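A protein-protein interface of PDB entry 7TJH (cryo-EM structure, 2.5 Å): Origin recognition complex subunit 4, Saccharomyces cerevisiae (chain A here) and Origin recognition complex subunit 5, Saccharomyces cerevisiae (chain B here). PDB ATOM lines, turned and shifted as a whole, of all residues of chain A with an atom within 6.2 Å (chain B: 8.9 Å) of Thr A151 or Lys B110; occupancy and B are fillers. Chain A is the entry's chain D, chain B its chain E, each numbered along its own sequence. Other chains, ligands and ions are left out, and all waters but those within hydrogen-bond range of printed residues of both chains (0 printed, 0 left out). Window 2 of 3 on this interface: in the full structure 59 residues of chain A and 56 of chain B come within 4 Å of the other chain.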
ATOM      1  N   ILE A 146       0.953  -3.268 -20.713  1.00  0.00           N
ATOM      2  CA  ILE A 146       1.185  -2.484 -19.501  1.00  0.00           C
ATOM      3  C   ILE A 146       0.067  -1.465 -19.301  1.00  0.00           C
ATOM      4  O   ILE A 146      -0.506  -1.348 -18.207  1.00  0.00           O
ATOM      5  CB  ILE A 146       2.568  -1.805 -19.567  1.00  0.00           C
ATOM      6  CG1 ILE A 146       3.695  -2.834 -19.756  1.00  0.00           C
ATOM      7  CG2 ILE A 146       2.815  -0.953 -18.338  1.00  0.00           C
ATOM      8  CD1 ILE A 146       3.625  -4.049 -18.841  1.00  0.00           C
ATOM      9  N   ASN A 147      -0.272  -0.730 -20.365  1.00  0.00           N
ATOM     10  CA  ASN A 147      -1.382   0.216 -20.317  1.00  0.00           C
ATOM     11  C   ASN A 147      -2.717  -0.485 -20.110  1.00  0.00           C
ATOM     12  O   ASN A 147      -3.590   0.053 -19.420  1.00  0.00           O
ATOM     13  CB  ASN A 147      -1.410   1.051 -21.595  1.00  0.00           C
ATOM     14  CG  ASN A 147      -0.227   1.988 -21.702  1.00  0.00           C
ATOM     15  OD1 ASN A 147       0.050   2.760 -20.787  1.00  0.00           O
ATOM     16  ND2 ASN A 147       0.485   1.917 -22.819  1.00  0.00           N
ATOM     17  N   GLY A 148      -2.879  -1.690 -20.671  1.00  0.00           N
ATOM     18  CA  GLY A 148      -4.087  -2.463 -20.432  1.00  0.00           C
ATOM     19  C   GLY A 148      -4.248  -2.870 -18.983  1.00  0.00           C
ATOM     20  O   GLY A 148      -5.333  -2.728 -18.410  1.00  0.00           O
ATOM     21  N   ILE A 149      -3.159  -3.338 -18.367  1.00  0.00           N
ATOM     22  CA  ILE A 149      -3.175  -3.719 -16.959  1.00  0.00           C
ATOM     23  C   ILE A 149      -3.474  -2.513 -16.076  1.00  0.00           C
ATOM     24  O   ILE A 149      -4.314  -2.590 -15.176  1.00  0.00           O
ATOM     25  CB  ILE A 149      -1.844  -4.396 -16.576  1.00  0.00           C
ATOM     26  CG1 ILE A 149      -1.784  -5.817 -17.138  1.00  0.00           C
ATOM     27  CG2 ILE A 149      -1.646  -4.436 -15.068  1.00  0.00           C
ATOM     28  CD1 ILE A 149      -0.393  -6.407 -17.129  1.00  0.00           C
ATOM     29  N   ALA A 150      -2.838  -1.369 -16.355  1.00  0.00           N
ATOM     30  CA  ALA A 150      -3.029  -0.198 -15.499  1.00  0.00           C
ATOM     31  C   ALA A 150      -4.431   0.398 -15.638  1.00  0.00           C
ATOM     32  O   ALA A 150      -5.055   0.775 -14.632  1.00  0.00           O
ATOM     33  CB  ALA A 150      -1.967   0.849 -15.810  1.00  0.00           C
ATOM     34  N   THR A 151      -4.948   0.466 -16.871  1.00  0.00           N
ATOM     35  CA  THR A 151      -6.302   0.961 -17.096  1.00  0.00           C
ATOM     36  C   THR A 151      -7.341   0.044 -16.461  1.00  0.00           C
ATOM     37  O   THR A 151      -8.279   0.523 -15.809  1.00  0.00           O
ATOM     38  CB  THR A 151      -6.554   1.116 -18.598  1.00  0.00           C
ATOM     39  OG1 THR A 151      -5.570   1.995 -19.154  1.00  0.00           O
ATOM     40  CG2 THR A 151      -7.937   1.692 -18.867  1.00  0.00           C
ATOM     41  N   GLN A 152      -7.163  -1.277 -16.597  1.00  0.00           N
ATOM     42  CA  GLN A 152      -8.094  -2.208 -15.969  1.00  0.00           C
ATOM     43  C   GLN A 152      -7.989  -2.176 -14.452  1.00  0.00           C
ATOM     44  O   GLN A 152      -9.010  -2.315 -13.770  1.00  0.00           O
ATOM     45  CB  GLN A 152      -7.868  -3.621 -16.499  1.00  0.00           C
ATOM     46  CG  GLN A 152      -8.426  -3.830 -17.891  1.00  0.00           C
ATOM     47  CD  GLN A 152      -8.134  -5.204 -18.439  1.00  0.00           C
ATOM     48  OE1 GLN A 152      -8.868  -6.156 -18.182  1.00  0.00           O
ATOM     49  NE2 GLN A 152      -7.053  -5.318 -19.198  1.00  0.00           N
ATOM     50  N   LEU A 153      -6.783  -1.948 -13.917  1.00  0.00           N
ATOM     51  CA  LEU A 153      -6.604  -1.811 -12.476  1.00  0.00           C
ATOM     52  C   LEU A 153      -7.372  -0.617 -11.935  1.00  0.00           C
ATOM     53  O   LEU A 153      -8.062  -0.734 -10.917  1.00  0.00           O
ATOM     54  CB  LEU A 153      -5.120  -1.680 -12.125  1.00  0.00           C
ATOM     55  CG  LEU A 153      -4.272  -2.935 -11.911  1.00  0.00           C
ATOM     56  CD1 LEU A 153      -2.796  -2.595 -11.993  1.00  0.00           C
ATOM     57  CD2 LEU A 153      -4.583  -3.601 -10.590  1.00  0.00           C
ATOM     58  N   GLU A 154      -7.308   0.528 -12.624  1.00  0.00           N
ATOM     59  CA  GLU A 154      -8.039   1.669 -12.082  1.00  0.00           C
ATOM     60  C   GLU A 154      -9.551   1.548 -12.284  1.00  0.00           C
ATOM     61  O   GLU A 154     -10.307   1.920 -11.375  1.00  0.00           O
ATOM     62  CB  GLU A 154      -7.520   2.996 -12.643  1.00  0.00           C
ATOM     63  CG  GLU A 154      -7.632   3.205 -14.125  1.00  0.00           C
ATOM     64  CD  GLU A 154      -7.281   4.619 -14.523  1.00  0.00           C
ATOM     65  OE1 GLU A 154      -7.998   5.551 -14.103  1.00  0.00           O
ATOM     66  OE2 GLU A 154      -6.295   4.804 -15.257  1.00  0.00           O
ATOM     67  N   GLN A 155     -10.028   0.968 -13.402  1.00  0.00           N
ATOM     68  CA  GLN A 155     -11.484   0.870 -13.530  1.00  0.00           C
ATOM     69  C   GLN A 155     -12.063  -0.257 -12.683  1.00  0.00           C
ATOM     70  O   GLN A 155     -13.270  -0.251 -12.421  1.00  0.00           O
ATOM     71  CB  GLN A 155     -11.946   0.678 -14.982  1.00  0.00           C
ATOM     72  CG  GLN A 155     -11.298  -0.436 -15.752  1.00  0.00           C
ATOM     73  CD  GLN A 155     -11.587  -0.379 -17.242  1.00  0.00           C
ATOM     74  OE1 GLN A 155     -11.624   0.695 -17.839  1.00  0.00           O
ATOM     75  NE2 GLN A 155     -11.811  -1.540 -17.846  1.00  0.00           N
ATOM     76  N   GLN A 156     -11.243  -1.213 -12.244  1.00  0.00           N
ATOM     77  CA  GLN A 156     -11.704  -2.212 -11.291  1.00  0.00           C
ATOM     78  C   GLN A 156     -11.624  -1.720  -9.854  1.00  0.00           C
ATOM     79  O   GLN A 156     -12.497  -2.057  -9.043  1.00  0.00           O
ATOM     80  CB  GLN A 156     -10.891  -3.503 -11.428  1.00  0.00           C
ATOM     81  CG  GLN A 156     -11.276  -4.374 -12.618  1.00  0.00           C
ATOM     82  CD  GLN A 156     -12.474  -5.253 -12.346  1.00  0.00           C
ATOM     83  OE1 GLN A 156     -12.463  -6.073 -11.433  1.00  0.00           O
ATOM     84  NE2 GLN A 156     -13.519  -5.087 -13.144  1.00  0.00           N
ATOM     85  N   GLN A 158     -11.881   1.465  -8.884  1.00  0.00           N
ATOM     86  CA  GLN A 158     -12.980   2.400  -8.668  1.00  0.00           C
ATOM     87  C   GLN A 158     -14.333   1.698  -8.680  1.00  0.00           C
ATOM     88  O   GLN A 158     -15.311   2.257  -8.173  1.00  0.00           O
ATOM     89  CB  GLN A 158     -12.941   3.530  -9.706  1.00  0.00           C
ATOM     90  CG  GLN A 158     -13.531   3.191 -11.061  1.00  0.00           C
ATOM     91  CD  GLN A 158     -13.222   4.243 -12.110  1.00  0.00           C
ATOM     92  OE1 GLN A 158     -12.338   4.062 -12.949  1.00  0.00           O
ATOM     93  NE2 GLN A 158     -13.956   5.350 -12.072  1.00  0.00           N
ATOM     94  N   SER A 176      -2.448   4.673 -14.318  1.00  0.00           N
ATOM     95  CA  SER A 176      -2.141   4.638 -15.743  1.00  0.00           C
ATOM     96  C   SER A 176      -1.665   5.974 -16.293  1.00  0.00           C
ATOM     97  O   SER A 176      -1.445   6.081 -17.504  1.00  0.00           O
ATOM     98  CB  SER A 176      -3.366   4.172 -16.534  1.00  0.00           C
ATOM     99  OG  SER A 176      -4.385   5.148 -16.504  1.00  0.00           O
ATOM    100  N   ALA B  78     -14.919   3.426 -34.344  1.00  0.00           N
ATOM    101  CA  ALA B  78     -15.201   4.340 -33.235  1.00  0.00           C
ATOM    102  C   ALA B  78     -16.079   5.513 -33.672  1.00  0.00           C
ATOM    103  O   ALA B  78     -17.076   5.831 -33.003  1.00  0.00           O
ATOM    104  CB  ALA B  78     -13.897   4.845 -32.625  1.00  0.00           C
ATOM    105  N   TYR B  97     -15.939  11.524 -27.881  1.00  0.00           N
ATOM    106  CA  TYR B  97     -14.567  11.051 -27.951  1.00  0.00           C
ATOM    107  C   TYR B  97     -14.060  11.191 -29.378  1.00  0.00           C
ATOM    108  O   TYR B  97     -14.816  11.002 -30.336  1.00  0.00           O
ATOM    109  CB  TYR B  97     -14.459   9.596 -27.487  1.00  0.00           C
ATOM    110  CG  TYR B  97     -14.781   9.414 -26.027  1.00  0.00           C
ATOM    111  CD1 TYR B  97     -13.806   9.591 -25.054  1.00  0.00           C
ATOM    112  CD2 TYR B  97     -16.067   9.087 -25.615  1.00  0.00           C
ATOM    113  CE1 TYR B  97     -14.097   9.434 -23.714  1.00  0.00           C
ATOM    114  CE2 TYR B  97     -16.370   8.931 -24.275  1.00  0.00           C
ATOM    115  CZ  TYR B  97     -15.382   9.109 -23.330  1.00  0.00           C
ATOM    116  OH  TYR B  97     -15.676   8.951 -21.994  1.00  0.00           O
ATOM    117  N   ASP B  98     -12.792  11.544 -29.513  1.00  0.00           N
ATOM    118  CA  ASP B  98     -12.193  11.719 -30.827  1.00  0.00           C
ATOM    119  C   ASP B  98     -11.818  10.359 -31.400  1.00  0.00           C
ATOM    120  O   ASP B  98     -11.068   9.618 -30.758  1.00  0.00           O
ATOM    121  CB  ASP B  98     -10.963  12.608 -30.726  1.00  0.00           C
ATOM    122  CG  ASP B  98     -10.381  12.963 -32.076  1.00  0.00           C
ATOM    123  OD1 ASP B  98     -11.112  12.930 -33.085  1.00  0.00           O
ATOM    124  OD2 ASP B  98      -9.178  13.273 -32.127  1.00  0.00           O
ATOM    125  N   GLN B 101      -8.002   9.305 -31.672  1.00  0.00           N
ATOM    126  CA  GLN B 101      -7.238   8.798 -30.538  1.00  0.00           C
ATOM    127  C   GLN B 101      -7.047   7.287 -30.597  1.00  0.00           C
ATOM    128  O   GLN B 101      -6.168   6.760 -29.909  1.00  0.00           O
ATOM    129  CB  GLN B 101      -7.919   9.186 -29.224  1.00  0.00           C
ATOM    130  CG  GLN B 101      -7.992  10.684 -28.989  1.00  0.00           C
ATOM    131  CD  GLN B 101      -7.342  11.109 -27.687  1.00  0.00           C
ATOM    132  OE1 GLN B 101      -6.302  10.581 -27.296  1.00  0.00           O
ATOM    133  NE2 GLN B 101      -7.955  12.070 -27.008  1.00  0.00           N
ATOM    134  N   VAL B 102      -7.844   6.583 -31.398  1.00  0.00           N
ATOM    135  CA  VAL B 102      -7.736   5.135 -31.533  1.00  0.00           C
ATOM    136  C   VAL B 102      -6.586   4.825 -32.488  1.00  0.00           C
ATOM    137  O   VAL B 102      -6.712   5.000 -33.702  1.00  0.00           O
ATOM    138  CB  VAL B 102      -9.049   4.520 -32.030  1.00  0.00           C
ATOM    139  CG1 VAL B 102      -8.918   3.010 -32.153  1.00  0.00           C
ATOM    140  CG2 VAL B 102     -10.190   4.887 -31.104  1.00  0.00           C
ATOM    141  N   GLU B 104      -4.476   1.824 -31.582  1.00  0.00           N
ATOM    142  CA  GLU B 104      -4.227   0.422 -31.288  1.00  0.00           C
ATOM    143  C   GLU B 104      -5.562  -0.286 -31.125  1.00  0.00           C
ATOM    144  O   GLU B 104      -6.589   0.366 -30.907  1.00  0.00           O
ATOM    145  CB  GLU B 104      -3.387   0.261 -30.006  1.00  0.00           C
ATOM    146  CG  GLU B 104      -2.038   0.994 -29.968  1.00  0.00           C
ATOM    147  CD  GLU B 104      -1.148   0.773 -31.190  1.00  0.00           C
ATOM    148  OE1 GLU B 104      -1.134  -0.337 -31.767  1.00  0.00           O
ATOM    149  OE2 GLU B 104      -0.396   1.710 -31.533  1.00  0.00           O
ATOM    150  N   PRO B 105      -5.596  -1.621 -31.280  1.00  0.00           N
ATOM    151  CA  PRO B 105      -6.818  -2.366 -30.911  1.00  0.00           C
ATOM    152  C   PRO B 105      -7.215  -2.209 -29.450  1.00  0.00           C
ATOM    153  O   PRO B 105      -8.413  -2.142 -29.137  1.00  0.00           O
ATOM    154  CB  PRO B 105      -6.455  -3.822 -31.240  1.00  0.00           C
ATOM    155  CG  PRO B 105      -5.369  -3.744 -32.228  1.00  0.00           C
ATOM    156  CD  PRO B 105      -4.638  -2.457 -32.029  1.00  0.00           C
ATOM    157  N   PHE B 106      -6.229  -2.136 -28.554  1.00  0.00           N
ATOM    158  CA  PHE B 106      -6.497  -1.864 -27.145  1.00  0.00           C
ATOM    159  C   PHE B 106      -7.124  -0.486 -26.951  1.00  0.00           C
ATOM    160  O   PHE B 106      -8.007  -0.311 -26.101  1.00  0.00           O
ATOM    161  CB  PHE B 106      -5.203  -2.010 -26.336  1.00  0.00           C
ATOM    162  CG  PHE B 106      -5.122  -1.101 -25.140  1.00  0.00           C
ATOM    163  CD1 PHE B 106      -5.806  -1.405 -23.974  1.00  0.00           C
ATOM    164  CD2 PHE B 106      -4.317   0.033 -25.168  1.00  0.00           C
ATOM    165  CE1 PHE B 106      -5.741  -0.564 -22.883  1.00  0.00           C
ATOM    166  CE2 PHE B 106      -4.237   0.869 -24.073  1.00  0.00           C
ATOM    167  CZ  PHE B 106      -4.943   0.566 -22.926  1.00  0.00           C
ATOM    168  N   LEU B 107      -6.674   0.501 -27.728  1.00  0.00           N
ATOM    169  CA  LEU B 107      -7.293   1.820 -27.683  1.00  0.00           C
ATOM    170  C   LEU B 107      -8.731   1.786 -28.185  1.00  0.00           C
ATOM    171  O   LEU B 107      -9.571   2.536 -27.680  1.00  0.00           O
ATOM    172  CB  LEU B 107      -6.451   2.815 -28.481  1.00  0.00           C
ATOM    173  CG  LEU B 107      -5.125   3.175 -27.803  1.00  0.00           C
ATOM    174  CD1 LEU B 107      -4.219   3.964 -28.731  1.00  0.00           C
ATOM    175  CD2 LEU B 107      -5.380   3.937 -26.512  1.00  0.00           C
ATOM    176  N   LEU B 108      -9.044   0.899 -29.139  1.00  0.00           N
ATOM    177  CA  LEU B 108     -10.433   0.719 -29.551  1.00  0.00           C
ATOM    178  C   LEU B 108     -11.267   0.098 -28.436  1.00  0.00           C
ATOM    179  O   LEU B 108     -12.421   0.496 -28.236  1.00  0.00           O
ATOM    180  CB  LEU B 108     -10.520  -0.132 -30.821  1.00  0.00           C
ATOM    181  CG  LEU B 108     -11.955  -0.329 -31.338  1.00  0.00           C
ATOM    182  CD1 LEU B 108     -12.506   0.961 -31.930  1.00  0.00           C
ATOM    183  CD2 LEU B 108     -12.079  -1.477 -32.319  1.00  0.00           C
ATOM    184  N   VAL B 109     -10.694  -0.861 -27.694  1.00  0.00           N
ATOM    185  CA  VAL B 109     -11.395  -1.457 -26.551  1.00  0.00           C
ATOM    186  C   VAL B 109     -11.700  -0.396 -25.496  1.00  0.00           C
ATOM    187  O   VAL B 109     -12.828  -0.298 -24.994  1.00  0.00           O
ATOM    188  CB  VAL B 109     -10.571  -2.611 -25.948  1.00  0.00           C
ATOM    189  CG1 VAL B 109     -11.268  -3.182 -24.722  1.00  0.00           C
ATOM    190  CG2 VAL B 109     -10.332  -3.704 -26.967  1.00  0.00           C
ATOM    191  N   LYS B 110     -10.702   0.438 -25.185  1.00  0.00           N
ATOM    192  CA  LYS B 110     -10.873   1.500 -24.195  1.00  0.00           C
ATOM    193  C   LYS B 110     -11.888   2.546 -24.652  1.00  0.00           C
ATOM    194  O   LYS B 110     -12.731   2.991 -23.861  1.00  0.00           O
ATOM    195  CB  LYS B 110      -9.521   2.152 -23.900  1.00  0.00           C
ATOM    196  CG  LYS B 110      -9.556   3.207 -22.808  1.00  0.00           C
ATOM    197  CD  LYS B 110      -8.164   3.518 -22.294  1.00  0.00           C
ATOM    198  CE  LYS B 110      -7.466   4.543 -23.171  1.00  0.00           C
ATOM    199  NZ  LYS B 110      -8.369   5.673 -23.518  1.00  0.00           N
ATOM    200  N   THR B 111     -11.838   2.931 -25.931  1.00  0.00           N
ATOM    201  CA  THR B 111     -12.755   3.940 -26.454  1.00  0.00           C
ATOM    202  C   THR B 111     -14.190   3.419 -26.507  1.00  0.00           C
ATOM    203  O   THR B 111     -15.125   4.146 -26.160  1.00  0.00           O
ATOM    204  CB  THR B 111     -12.283   4.395 -27.836  1.00  0.00           C
ATOM    205  OG1 THR B 111     -10.930   4.859 -27.747  1.00  0.00           O
ATOM    206  CG2 THR B 111     -13.149   5.519 -28.373  1.00  0.00           C
ATOM    207  N   LEU B 112     -14.381   2.155 -26.899  1.00  0.00           N
ATOM    208  CA  LEU B 112     -15.723   1.575 -26.905  1.00  0.00           C
ATOM    209  C   LEU B 112     -16.264   1.403 -25.490  1.00  0.00           C
ATOM    210  O   LEU B 112     -17.464   1.584 -25.265  1.00  0.00           O
ATOM    211  CB  LEU B 112     -15.726   0.238 -27.647  1.00  0.00           C
ATOM    212  CG  LEU B 112     -15.587   0.290 -29.172  1.00  0.00           C
ATOM    213  CD1 LEU B 112     -15.570  -1.110 -29.755  1.00  0.00           C
ATOM    214  CD2 LEU B 112     -16.686   1.132 -29.809  1.00  0.00           C
ATOM    215  N   HIS B 113     -15.395   1.068 -24.530  1.00  0.00           N
ATOM    216  CA  HIS B 113     -15.795   0.996 -23.124  1.00  0.00           C
ATOM    217  C   HIS B 113     -16.267   2.365 -22.632  1.00  0.00           C
ATOM    218  O   HIS B 113     -17.322   2.482 -21.991  1.00  0.00           O
ATOM    219  CB  HIS B 113     -14.598   0.474 -22.312  1.00  0.00           C
ATOM    220  CG  HIS B 113     -14.883   0.111 -20.881  1.00  0.00           C
ATOM    221  ND1 HIS B 113     -15.935   0.616 -20.146  1.00  0.00           N
ATOM    222  CD2 HIS B 113     -14.205  -0.705 -20.038  1.00  0.00           C
ATOM    223  CE1 HIS B 113     -15.901   0.117 -18.924  1.00  0.00           C
ATOM    224  NE2 HIS B 113     -14.859  -0.686 -18.831  1.00  0.00           N
ATOM    225  N   ASN B 114     -15.507   3.416 -22.959  1.00  0.00           N
ATOM    226  CA  ASN B 114     -15.858   4.764 -22.525  1.00  0.00           C
ATOM    227  C   ASN B 114     -17.121   5.279 -23.212  1.00  0.00           C
ATOM    228  O   ASN B 114     -17.886   6.035 -22.605  1.00  0.00           O
ATOM    229  CB  ASN B 114     -14.682   5.709 -22.777  1.00  0.00           C
ATOM    230  CG  ASN B 114     -13.527   5.469 -21.827  1.00  0.00           C
ATOM    231  OD1 ASN B 114     -13.705   4.938 -20.732  1.00  0.00           O
ATOM    232  ND2 ASN B 114     -12.328   5.851 -22.248  1.00  0.00           N
ATOM    233  N   ILE B 115     -17.347   4.897 -24.471  1.00  0.00           N
ATOM    234  CA  ILE B 115     -18.579   5.272 -25.159  1.00  0.00           C
ATOM    235  C   ILE B 115     -19.773   4.509 -24.584  1.00  0.00           C
ATOM    236  O   ILE B 115     -20.854   5.075 -24.400  1.00  0.00           O
ATOM    237  CB  ILE B 115     -18.423   5.056 -26.680  1.00  0.00           C
ATOM    238  CG1 ILE B 115     -17.473   6.093 -27.274  1.00  0.00           C
ATOM    239  CG2 ILE B 115     -19.753   5.150 -27.422  1.00  0.00           C
ATOM    240  CD1 ILE B 115     -16.880   5.668 -28.591  1.00  0.00           C
ATOM    241  N   PHE B 116     -19.596   3.227 -24.260  1.00  0.00           N
ATOM    242  CA  PHE B 116     -20.729   2.421 -23.821  1.00  0.00           C
ATOM    243  C   PHE B 116     -21.122   2.676 -22.370  1.00  0.00           C
ATOM    244  O   PHE B 116     -22.275   2.416 -22.009  1.00  0.00           O
ATOM    245  CB  PHE B 116     -20.444   0.924 -24.001  1.00  0.00           C
ATOM    246  CG  PHE B 116     -20.333   0.477 -25.440  1.00  0.00           C
ATOM    247  CD1 PHE B 116     -20.816   1.259 -26.481  1.00  0.00           C
ATOM    248  CD2 PHE B 116     -19.727  -0.733 -25.746  1.00  0.00           C
ATOM    249  CE1 PHE B 116     -20.695   0.844 -27.791  1.00  0.00           C
ATOM    250  CE2 PHE B 116     -19.607  -1.153 -27.058  1.00  0.00           C
ATOM    251  CZ  PHE B 116     -20.094  -0.364 -28.080  1.00  0.00           C
ATOM    252  N   VAL B 117     -20.209   3.174 -21.526  1.00  0.00           N
ATOM    253  CA  VAL B 117     -20.591   3.396 -20.128  1.00  0.00           C
ATOM    254  C   VAL B 117     -21.466   4.621 -19.912  1.00  0.00           C
ATOM    255  O   VAL B 117     -22.005   4.790 -18.812  1.00  0.00           O
ATOM    256  CB  VAL B 117     -19.395   3.546 -19.169  1.00  0.00           C
ATOM    257  CG1 VAL B 117     -18.731   2.206 -18.941  1.00  0.00           C
ATOM    258  CG2 VAL B 117     -18.412   4.580 -19.675  1.00  0.00           C
ATOM    259  N   LEU B 152     -12.536  -9.507 -29.925  1.00  0.00           N
ATOM    260  CA  LEU B 152     -12.816  -8.173 -29.398  1.00  0.00           C
ATOM    261  C   LEU B 152     -13.970  -8.159 -28.397  1.00  0.00           C
ATOM    262  O   LEU B 152     -13.972  -7.331 -27.480  1.00  0.00           O
ATOM    263  CB  LEU B 152     -13.086  -7.225 -30.578  1.00  0.00           C
ATOM    264  CG  LEU B 152     -13.479  -5.735 -30.551  1.00  0.00           C
ATOM    265  CD1 LEU B 152     -14.951  -5.439 -30.239  1.00  0.00           C
ATOM    266  CD2 LEU B 152     -12.589  -4.981 -29.598  1.00  0.00           C
ATOM    267  N   LEU B 155     -13.276  -8.555 -24.436  1.00  0.00           N
ATOM    268  CA  LEU B 155     -12.681  -7.478 -23.658  1.00  0.00           C
ATOM    269  C   LEU B 155     -13.662  -6.364 -23.320  1.00  0.00           C
ATOM    270  O   LEU B 155     -13.363  -5.543 -22.446  1.00  0.00           O
ATOM    271  CB  LEU B 155     -11.481  -6.881 -24.401  1.00  0.00           C
ATOM    272  CG  LEU B 155     -10.343  -7.817 -24.804  1.00  0.00           C
ATOM    273  CD1 LEU B 155      -9.156  -7.002 -25.274  1.00  0.00           C
ATOM    274  CD2 LEU B 155      -9.941  -8.740 -23.667  1.00  0.00           C
ATOM    275  N   LEU B 156     -14.806  -6.313 -23.987  1.00  0.00           N
ATOM    276  CA  LEU B 156     -15.851  -5.361 -23.664  1.00  0.00           C
ATOM    277  C   LEU B 156     -16.622  -5.832 -22.433  1.00  0.00           C
ATOM    278  O   LEU B 156     -16.599  -7.020 -22.103  1.00  0.00           O
ATOM    279  CB  LEU B 156     -16.769  -5.185 -24.871  1.00  0.00           C
ATOM    280  CG  LEU B 156     -16.082  -4.472 -26.036  1.00  0.00           C
ATOM    281  CD1 LEU B 156     -16.981  -4.422 -27.247  1.00  0.00           C
ATOM    282  CD2 LEU B 156     -15.644  -3.070 -25.625  1.00  0.00           C
ATOM    283  N   PRO B 157     -17.264  -4.914 -21.698  1.00  0.00           N
ATOM    284  CA  PRO B 157     -18.018  -5.326 -20.506  1.00  0.00           C
ATOM    285  C   PRO B 157     -19.212  -6.210 -20.835  1.00  0.00           C
ATOM    286  O   PRO B 157     -19.881  -6.050 -21.858  1.00  0.00           O
ATOM    287  CB  PRO B 157     -18.468  -3.994 -19.894  1.00  0.00           C
ATOM    288  CG  PRO B 157     -18.353  -3.007 -20.990  1.00  0.00           C
ATOM    289  CD  PRO B 157     -17.173  -3.446 -21.777  1.00  0.00           C
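Thr A151 touches just one residue of chain B: Lys B110 (3.9 Å).
Lys B110 touches just one residue of chain A: Thr A151.
No residue of chain B comes within 4 Å of Ala A150.
Of the printed residues of chain B, Gln A155 touches His B113.
Of the printed residues of chain A, Phe B106 touches Asn A147 and Gly A148.
Of the printed residues of chain A, His B113 touches Gln A155.
The nearest residue of chain B that does not touch Thr A151 is Phe B106 (4.1 Å).
The nearest residue of chain A that does not touch Lys B110 is Gln A155 (5.9 Å).
CZ of Phe B106 touches C of Asn A147, at 3.7 Å.
Phe B106 touches Gly A148.
Lys B110 touches Thr A151 (CD to CG2, 3.9 Å).
Of the 23 printed residues of chain B, 3 touch a printed residue of chain A.
Printed residues of chain B that touch a printed residue of chain A: Phe B106, Lys B110 and His B113.
Hydrophobic or aromatic side chains of chain B within 4 Å of the printed part of chain A: Phe B106 and His B113.
Along chain B the printed residues that touch a printed residue of chain A span positions 106 to 113.
Of the 13 printed residues of chain A, 4 touch a printed residue of chain B.
Among the printed residues, 4 pairs touch across the chains.
The backbone carbonyl oxygen (O) of Lys B110 sits close to the side-chain amide nitrogen (ND2) of Asn B114 (3.3 Å).
O of Asn A147 lies within hydrogen-bond range of OG1 of Thr A151, at 2.8 Å.
The side-chain amide nitrogen (NE2) of Gln A152 lies within hydrogen-bond range of the backbone carbonyl oxygen (O) of Gly A148, at 3.2 Å.
The side-chain amide nitrogen (NE2) of Gln A155 sits at hydrogen-bond distance from a ring nitrogen (NE2) of His B113 (3.3 Å).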
